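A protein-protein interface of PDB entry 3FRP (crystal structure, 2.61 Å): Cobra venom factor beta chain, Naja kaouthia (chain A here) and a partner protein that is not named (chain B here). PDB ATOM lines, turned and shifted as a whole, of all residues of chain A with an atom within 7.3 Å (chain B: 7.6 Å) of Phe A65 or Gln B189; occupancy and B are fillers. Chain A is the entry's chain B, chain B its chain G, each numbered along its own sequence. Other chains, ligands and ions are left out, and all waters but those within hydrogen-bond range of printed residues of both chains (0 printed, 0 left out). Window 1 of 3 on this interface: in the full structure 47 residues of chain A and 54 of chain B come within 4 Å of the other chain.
O of Ile A62 touches CA of Val B193 (3.2 Å).
Ile A62 touches Lys B230.
Leu A63 touches Ile B192.
Val B193 touches Leu A63.
Thr A64 touches Lys B190 (O to O, 3.7 Å).
Gln B189 touches Phe A65 (NE2 to CD2, 3.7 Å).
O of Lys B190 touches CA of Phe A65, at 3.3 Å.
Tyr A66 touches Gln B189.
Pro B185 touches Asn A67 (CB to OD1, 3.4 Å).
Asn A67 touches Gly B187 (OD1 to C, 3.5 Å).
Printed residues of chain B that touch a printed residue of chain A: Pro B185, Gly B187, Val B188, Gln B189, Lys B190, Ser B191, Ile B192, Val B193, Thr B194, Thr B225, Ile B227, Glu B228, Thr B229 and Lys B230.
Hydrophobic or aromatic side chains of chain B within 4 Å of the printed part of chain A: Pro B185, Ile B192, Val B193 and Ile B227.
Of the 7 printed residues of chain A, 7 touch a printed residue of chain B.
Hydrophobic or aromatic side chains of chain A within 4 Å of the printed part of chain B: Ile A62, Leu A63, Phe A65, Tyr A66 and Ala A68.
The backbone NH (N) of Thr B194 sits at hydrogen-bond distance from the backbone carbonyl oxygen (O) of Ile A62 (2.8 Å).
The backbone NH (N) of Lys B230 sits at hydrogen-bond distance from the backbone carbonyl oxygen (O) of Leu A63, at 3.1 Å.
The backbone NH (N) of Lys B190 lies within hydrogen-bond range of the backbone carbonyl oxygen (O) of Tyr A66.
O of Glu B228 lies within hydrogen-bond range of N of Phe A65.
OG1 of Thr B194 sits at hydrogen-bond distance from OG1 of Thr A64 (3.1 Å).
The backbone carbonyl oxygen of Ile B192 lies within hydrogen-bond range of the backbone NH of Thr A64, 3.0 Å away.
The backbone carbonyl oxygen of Ala A68 sits at hydrogen-bond distance from the backbone NH of Val B188 (3.4 Å).
Phe A65 touches just these residues of chain B: Gln B189, Lys B190, Ser B191, Ile B227 and Glu B228.
Of chain A, only Phe A65 (3.7 Å) and Tyr A66 (3.6 Å) come within 4 Å of Gln B189.
Of the printed residues of chain A, Pro B185 touches Asn A67 (3.4 Å).
Printed residues of chain B within 4 Å of Tyr A66: Gln B189 (3.6 Å), Lys B190 (2.9 Å), Ile B192 (3.8 Å) and Ile B227 (3.8 Å).
Printed residues of chain A within 4 Å of Gly B187: Asn A67 (3.5 Å) and Ala A68 (3.9 Å).
Printed residues of chain A within 4 Å of Ile B227: Phe A65 and Tyr A66.
Printed residues of chain B within 4 Å of Asn A67: Pro B185, Gly B187 and Thr B225.
Glu B186 touches none of the printed residues of chain A.
Glu B226 touches none of the printed residues of chain A.
The nearest residue of chain A that does not touch Gln B189 is Asn A67 (4.04 Å).
The nearest printed residue of chain B that does not touch Ile A62 is Thr B229 (5.4 Å).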
ATOM      1  N   ILE A  62      -3.499  20.030  -4.232  1.00  0.00           N
ATOM      2  CA  ILE A  62      -3.284  19.325  -2.961  1.00  0.00           C
ATOM      3  C   ILE A  62      -4.506  19.437  -2.045  1.00  0.00           C
ATOM      4  O   ILE A  62      -5.093  20.510  -1.921  1.00  0.00           O
ATOM      5  CB  ILE A  62      -2.050  19.878  -2.213  1.00  0.00           C
ATOM      6  CG1 ILE A  62      -0.851  20.024  -3.166  1.00  0.00           C
ATOM      7  CG2 ILE A  62      -1.726  19.038  -0.962  1.00  0.00           C
ATOM      8  CD1 ILE A  62      -0.429  18.738  -3.885  1.00  0.00           C
ATOM      9  N   LEU A  63      -4.866  18.326  -1.400  1.00  0.00           N
ATOM     10  CA  LEU A  63      -6.066  18.231  -0.555  1.00  0.00           C
ATOM     11  C   LEU A  63      -5.684  17.754   0.848  1.00  0.00           C
ATOM     12  O   LEU A  63      -4.883  16.836   0.980  1.00  0.00           O
ATOM     13  CB  LEU A  63      -7.075  17.270  -1.198  1.00  0.00           C
ATOM     14  CG  LEU A  63      -7.424  17.532  -2.675  1.00  0.00           C
ATOM     15  CD1 LEU A  63      -7.641  16.237  -3.438  1.00  0.00           C
ATOM     16  CD2 LEU A  63      -8.624  18.469  -2.826  1.00  0.00           C
ATOM     17  N   THR A  64      -6.244  18.385   1.882  1.00  0.00           N
ATOM     18  CA  THR A  64      -5.896  18.083   3.283  1.00  0.00           C
ATOM     19  C   THR A  64      -7.112  18.145   4.237  1.00  0.00           C
ATOM     20  O   THR A  64      -7.462  19.208   4.765  1.00  0.00           O
ATOM     21  CB  THR A  64      -4.728  18.991   3.801  1.00  0.00           C
ATOM     22  OG1 THR A  64      -3.638  18.975   2.865  1.00  0.00           O
ATOM     23  CG2 THR A  64      -4.206  18.521   5.166  1.00  0.00           C
ATOM     24  N   PHE A  65      -7.737  16.986   4.456  1.00  0.00           N
ATOM     25  CA  PHE A  65      -8.950  16.857   5.267  1.00  0.00           C
ATOM     26  C   PHE A  65      -8.569  16.566   6.692  1.00  0.00           C
ATOM     27  O   PHE A  65      -7.658  15.786   6.944  1.00  0.00           O
ATOM     28  CB  PHE A  65      -9.804  15.688   4.781  1.00  0.00           C
ATOM     29  CG  PHE A  65      -9.945  15.613   3.294  1.00  0.00           C
ATOM     30  CD1 PHE A  65      -8.876  15.203   2.500  1.00  0.00           C
ATOM     31  CD2 PHE A  65     -11.156  15.926   2.687  1.00  0.00           C
ATOM     32  CE1 PHE A  65      -9.001  15.128   1.128  1.00  0.00           C
ATOM     33  CE2 PHE A  65     -11.293  15.843   1.311  1.00  0.00           C
ATOM     34  CZ  PHE A  65     -10.211  15.445   0.529  1.00  0.00           C
ATOM     35  N   TYR A  66      -9.286  17.171   7.626  1.00  0.00           N
ATOM     36  CA  TYR A  66      -9.034  16.949   9.045  1.00  0.00           C
ATOM     37  C   TYR A  66     -10.348  17.126   9.773  1.00  0.00           C
ATOM     38  O   TYR A  66     -11.269  17.762   9.253  1.00  0.00           O
ATOM     39  CB  TYR A  66      -7.982  17.943   9.576  1.00  0.00           C
ATOM     40  CG  TYR A  66      -8.465  19.374   9.658  1.00  0.00           C
ATOM     41  CD1 TYR A  66      -8.726  19.970  10.885  1.00  0.00           C
ATOM     42  CD2 TYR A  66      -8.682  20.121   8.503  1.00  0.00           C
ATOM     43  CE1 TYR A  66      -9.184  21.277  10.962  1.00  0.00           C
ATOM     44  CE2 TYR A  66      -9.140  21.432   8.567  1.00  0.00           C
ATOM     45  CZ  TYR A  66      -9.391  22.004   9.799  1.00  0.00           C
ATOM     46  OH  TYR A  66      -9.846  23.303   9.858  1.00  0.00           O
ATOM     47  N   ASN A  67     -10.457  16.569  10.969  1.00  0.00           N
ATOM     48  CA  ASN A  67     -11.637  16.863  11.760  1.00  0.00           C
ATOM     49  C   ASN A  67     -11.513  18.187  12.521  1.00  0.00           C
ATOM     50  O   ASN A  67     -10.796  18.301  13.528  1.00  0.00           O
ATOM     51  CB  ASN A  67     -12.064  15.681  12.650  1.00  0.00           C
ATOM     52  CG  ASN A  67     -13.216  14.869  12.037  1.00  0.00           C
ATOM     53  OD1 ASN A  67     -14.311  14.795  12.610  1.00  0.00           O
ATOM     54  ND2 ASN A  67     -12.974  14.277  10.863  1.00  0.00           N
ATOM     55  N   ALA A  68     -12.190  19.195  11.976  1.00  0.00           N
ATOM     56  CA  ALA A  68     -12.370  20.482  12.633  1.00  0.00           C
ATOM     57  C   ALA A  68     -13.549  20.384  13.607  1.00  0.00           C
ATOM     58  O   ALA A  68     -14.467  19.576  13.414  1.00  0.00           O
ATOM     59  CB  ALA A  68     -12.609  21.584  11.591  1.00  0.00           C
ATOM     60  N   PRO B 185     -15.480   9.987  14.397  1.00  0.00           N
ATOM     61  CA  PRO B 185     -15.147  11.213  15.136  1.00  0.00           C
ATOM     62  C   PRO B 185     -16.307  12.188  15.345  1.00  0.00           C
ATOM     63  O   PRO B 185     -17.165  12.329  14.477  1.00  0.00           O
ATOM     64  CB  PRO B 185     -14.078  11.871  14.254  1.00  0.00           C
ATOM     65  CG  PRO B 185     -13.561  10.789  13.347  1.00  0.00           C
ATOM     66  CD  PRO B 185     -14.305   9.515  13.643  1.00  0.00           C
ATOM     67  N   GLU B 186     -16.284  12.877  16.485  1.00  0.00           N
ATOM     68  CA  GLU B 186     -17.374  13.743  16.937  1.00  0.00           C
ATOM     69  C   GLU B 186     -17.636  14.981  16.061  1.00  0.00           C
ATOM     70  O   GLU B 186     -18.705  15.600  16.174  1.00  0.00           O
ATOM     71  CB  GLU B 186     -17.157  14.149  18.414  1.00  0.00           C
ATOM     72  CG  GLU B 186     -18.453  14.307  19.236  1.00  0.00           C
ATOM     73  CD  GLU B 186     -18.212  14.565  20.733  1.00  0.00           C
ATOM     74  OE1 GLU B 186     -18.450  15.714  21.177  1.00  0.00           O
ATOM     75  OE2 GLU B 186     -17.791  13.637  21.474  1.00  0.00           O
ATOM     76  N   GLY B 187     -16.694  15.332  15.181  1.00  0.00           N
ATOM     77  CA  GLY B 187     -16.780  16.598  14.434  1.00  0.00           C
ATOM     78  C   GLY B 187     -17.279  16.574  12.991  1.00  0.00           C
ATOM     79  O   GLY B 187     -17.821  15.572  12.518  1.00  0.00           O
ATOM     80  N   VAL B 188     -17.102  17.705  12.304  1.00  0.00           N
ATOM     81  CA  VAL B 188     -17.381  17.821  10.863  1.00  0.00           C
ATOM     82  C   VAL B 188     -16.086  17.939  10.062  1.00  0.00           C
ATOM     83  O   VAL B 188     -15.302  18.871  10.264  1.00  0.00           O
ATOM     84  CB  VAL B 188     -18.251  19.048  10.517  1.00  0.00           C
ATOM     85  CG1 VAL B 188     -19.021  18.783   9.217  1.00  0.00           C
ATOM     86  CG2 VAL B 188     -19.185  19.431  11.681  1.00  0.00           C
ATOM     87  N   GLN B 189     -15.887  16.992   9.151  1.00  0.00           N
ATOM     88  CA  GLN B 189     -14.684  16.909   8.319  1.00  0.00           C
ATOM     89  C   GLN B 189     -14.526  18.171   7.463  1.00  0.00           C
ATOM     90  O   GLN B 189     -15.443  18.528   6.729  1.00  0.00           O
ATOM     91  CB  GLN B 189     -14.782  15.654   7.447  1.00  0.00           C
ATOM     92  CG  GLN B 189     -13.699  15.481   6.395  1.00  0.00           C
ATOM     93  CD  GLN B 189     -14.187  14.668   5.200  1.00  0.00           C
ATOM     94  OE1 GLN B 189     -15.307  14.858   4.717  1.00  0.00           O
ATOM     95  NE2 GLN B 189     -13.344  13.763   4.717  1.00  0.00           N
ATOM     96  N   LYS B 190     -13.374  18.839   7.574  1.00  0.00           N
ATOM     97  CA  LYS B 190     -13.106  20.119   6.878  1.00  0.00           C
ATOM     98  C   LYS B 190     -12.012  19.983   5.798  1.00  0.00           C
ATOM     99  O   LYS B 190     -10.961  19.363   6.021  1.00  0.00           O
ATOM    100  CB  LYS B 190     -12.758  21.219   7.892  1.00  0.00           C
ATOM    101  CG  LYS B 190     -12.419  22.606   7.324  1.00  0.00           C
ATOM    102  CD  LYS B 190     -13.556  23.603   7.506  1.00  0.00           C
ATOM    103  CE  LYS B 190     -13.109  25.013   7.149  1.00  0.00           C
ATOM    104  NZ  LYS B 190     -14.282  25.906   6.923  1.00  0.00           N
ATOM    105  N   SER B 191     -12.268  20.589   4.640  1.00  0.00           N
ATOM    106  CA  SER B 191     -11.533  20.283   3.411  1.00  0.00           C
ATOM    107  C   SER B 191     -10.781  21.491   2.811  1.00  0.00           C
ATOM    108  O   SER B 191     -11.397  22.411   2.252  1.00  0.00           O
ATOM    109  CB  SER B 191     -12.501  19.662   2.386  1.00  0.00           C
ATOM    110  OG  SER B 191     -11.830  18.888   1.401  1.00  0.00           O
ATOM    111  N   ILE B 192      -9.451  21.465   2.928  1.00  0.00           N
ATOM    112  CA  ILE B 192      -8.574  22.517   2.397  1.00  0.00           C
ATOM    113  C   ILE B 192      -7.877  22.078   1.097  1.00  0.00           C
ATOM    114  O   ILE B 192      -7.120  21.107   1.085  1.00  0.00           O
ATOM    115  CB  ILE B 192      -7.475  22.955   3.428  1.00  0.00           C
ATOM    116  CG1 ILE B 192      -8.038  23.062   4.854  1.00  0.00           C
ATOM    117  CG2 ILE B 192      -6.824  24.269   2.997  1.00  0.00           C
ATOM    118  CD1 ILE B 192      -6.975  23.074   5.954  1.00  0.00           C
ATOM    119  N   VAL B 193      -8.148  22.786   0.003  1.00  0.00           N
ATOM    120  CA  VAL B 193      -7.307  22.682  -1.189  1.00  0.00           C
ATOM    121  C   VAL B 193      -6.083  23.552  -0.890  1.00  0.00           C
ATOM    122  O   VAL B 193      -6.126  24.777  -1.042  1.00  0.00           O
ATOM    123  CB  VAL B 193      -8.047  23.098  -2.516  1.00  0.00           C
ATOM    124  CG1 VAL B 193      -7.081  23.202  -3.693  1.00  0.00           C
ATOM    125  CG2 VAL B 193      -9.169  22.109  -2.858  1.00  0.00           C
ATOM    126  N   THR B 194      -5.013  22.900  -0.422  1.00  0.00           N
ATOM    127  CA  THR B 194      -3.778  23.572   0.037  1.00  0.00           C
ATOM    128  C   THR B 194      -3.175  24.546  -0.978  1.00  0.00           C
ATOM    129  O   THR B 194      -2.636  25.590  -0.590  1.00  0.00           O
ATOM    130  CB  THR B 194      -2.704  22.562   0.495  1.00  0.00           C
ATOM    131  OG1 THR B 194      -3.251  21.716   1.512  1.00  0.00           O
ATOM    132  CG2 THR B 194      -1.461  23.289   1.044  1.00  0.00           C
ATOM    133  N   THR B 225      -9.127  12.425  15.505  1.00  0.00           N
ATOM    134  CA  THR B 225      -9.078  13.037  14.187  1.00  0.00           C
ATOM    135  C   THR B 225      -7.805  12.624  13.459  1.00  0.00           C
ATOM    136  O   THR B 225      -6.715  13.078  13.804  1.00  0.00           O
ATOM    137  CB  THR B 225      -9.161  14.562  14.305  1.00  0.00           C
ATOM    138  N   GLU B 226      -7.943  11.743  12.472  1.00  0.00           N
ATOM    139  CA  GLU B 226      -6.829  11.389  11.599  1.00  0.00           C
ATOM    140  C   GLU B 226      -6.910  12.266  10.357  1.00  0.00           C
ATOM    141  O   GLU B 226      -7.885  12.997  10.175  1.00  0.00           O
ATOM    142  CB  GLU B 226      -6.852   9.906  11.215  1.00  0.00           C
ATOM    143  CG  GLU B 226      -5.451   9.308  10.976  1.00  0.00           C
ATOM    144  CD  GLU B 226      -5.382   8.329   9.795  1.00  0.00           C
ATOM    145  OE1 GLU B 226      -6.356   8.242   9.013  1.00  0.00           O
ATOM    146  OE2 GLU B 226      -4.333   7.652   9.640  1.00  0.00           O
ATOM    147  N   ILE B 227      -5.882  12.188   9.514  1.00  0.00           N
ATOM    148  CA  ILE B 227      -5.683  13.131   8.408  1.00  0.00           C
ATOM    149  C   ILE B 227      -5.258  12.408   7.119  1.00  0.00           C
ATOM    150  O   ILE B 227      -4.410  11.502   7.151  1.00  0.00           O
ATOM    151  CB  ILE B 227      -4.573  14.180   8.769  1.00  0.00           C
ATOM    152  CG1 ILE B 227      -4.491  14.461  10.292  1.00  0.00           C
ATOM    153  CG2 ILE B 227      -4.682  15.447   7.915  1.00  0.00           C
ATOM    154  CD1 ILE B 227      -5.629  15.310  10.905  1.00  0.00           C
ATOM    155  N   GLU B 228      -5.847  12.805   5.991  1.00  0.00           N
ATOM    156  CA  GLU B 228      -5.389  12.333   4.672  1.00  0.00           C
ATOM    157  C   GLU B 228      -4.978  13.501   3.772  1.00  0.00           C
ATOM    158  O   GLU B 228      -5.469  14.621   3.934  1.00  0.00           O
ATOM    159  CB  GLU B 228      -6.445  11.466   3.992  1.00  0.00           C
ATOM    160  N   THR B 229      -4.070  13.239   2.833  1.00  0.00           N
ATOM    161  CA  THR B 229      -3.591  14.269   1.908  1.00  0.00           C
ATOM    162  C   THR B 229      -3.394  13.737   0.478  1.00  0.00           C
ATOM    163  O   THR B 229      -2.482  12.956   0.220  1.00  0.00           O
ATOM    164  CB  THR B 229      -2.303  14.915   2.452  1.00  0.00           C
ATOM    165  N   LYS B 230      -4.254  14.159  -0.443  1.00  0.00           N
ATOM    166  CA  LYS B 230      -4.217  13.655  -1.829  1.00  0.00           C
ATOM    167  C   LYS B 230      -3.375  14.536  -2.788  1.00  0.00           C
ATOM    168  O   LYS B 230      -3.480  15.767  -2.768  1.00  0.00           O
ATOM    169  CB  LYS B 230      -5.648  13.453  -2.359  1.00  0.00           C
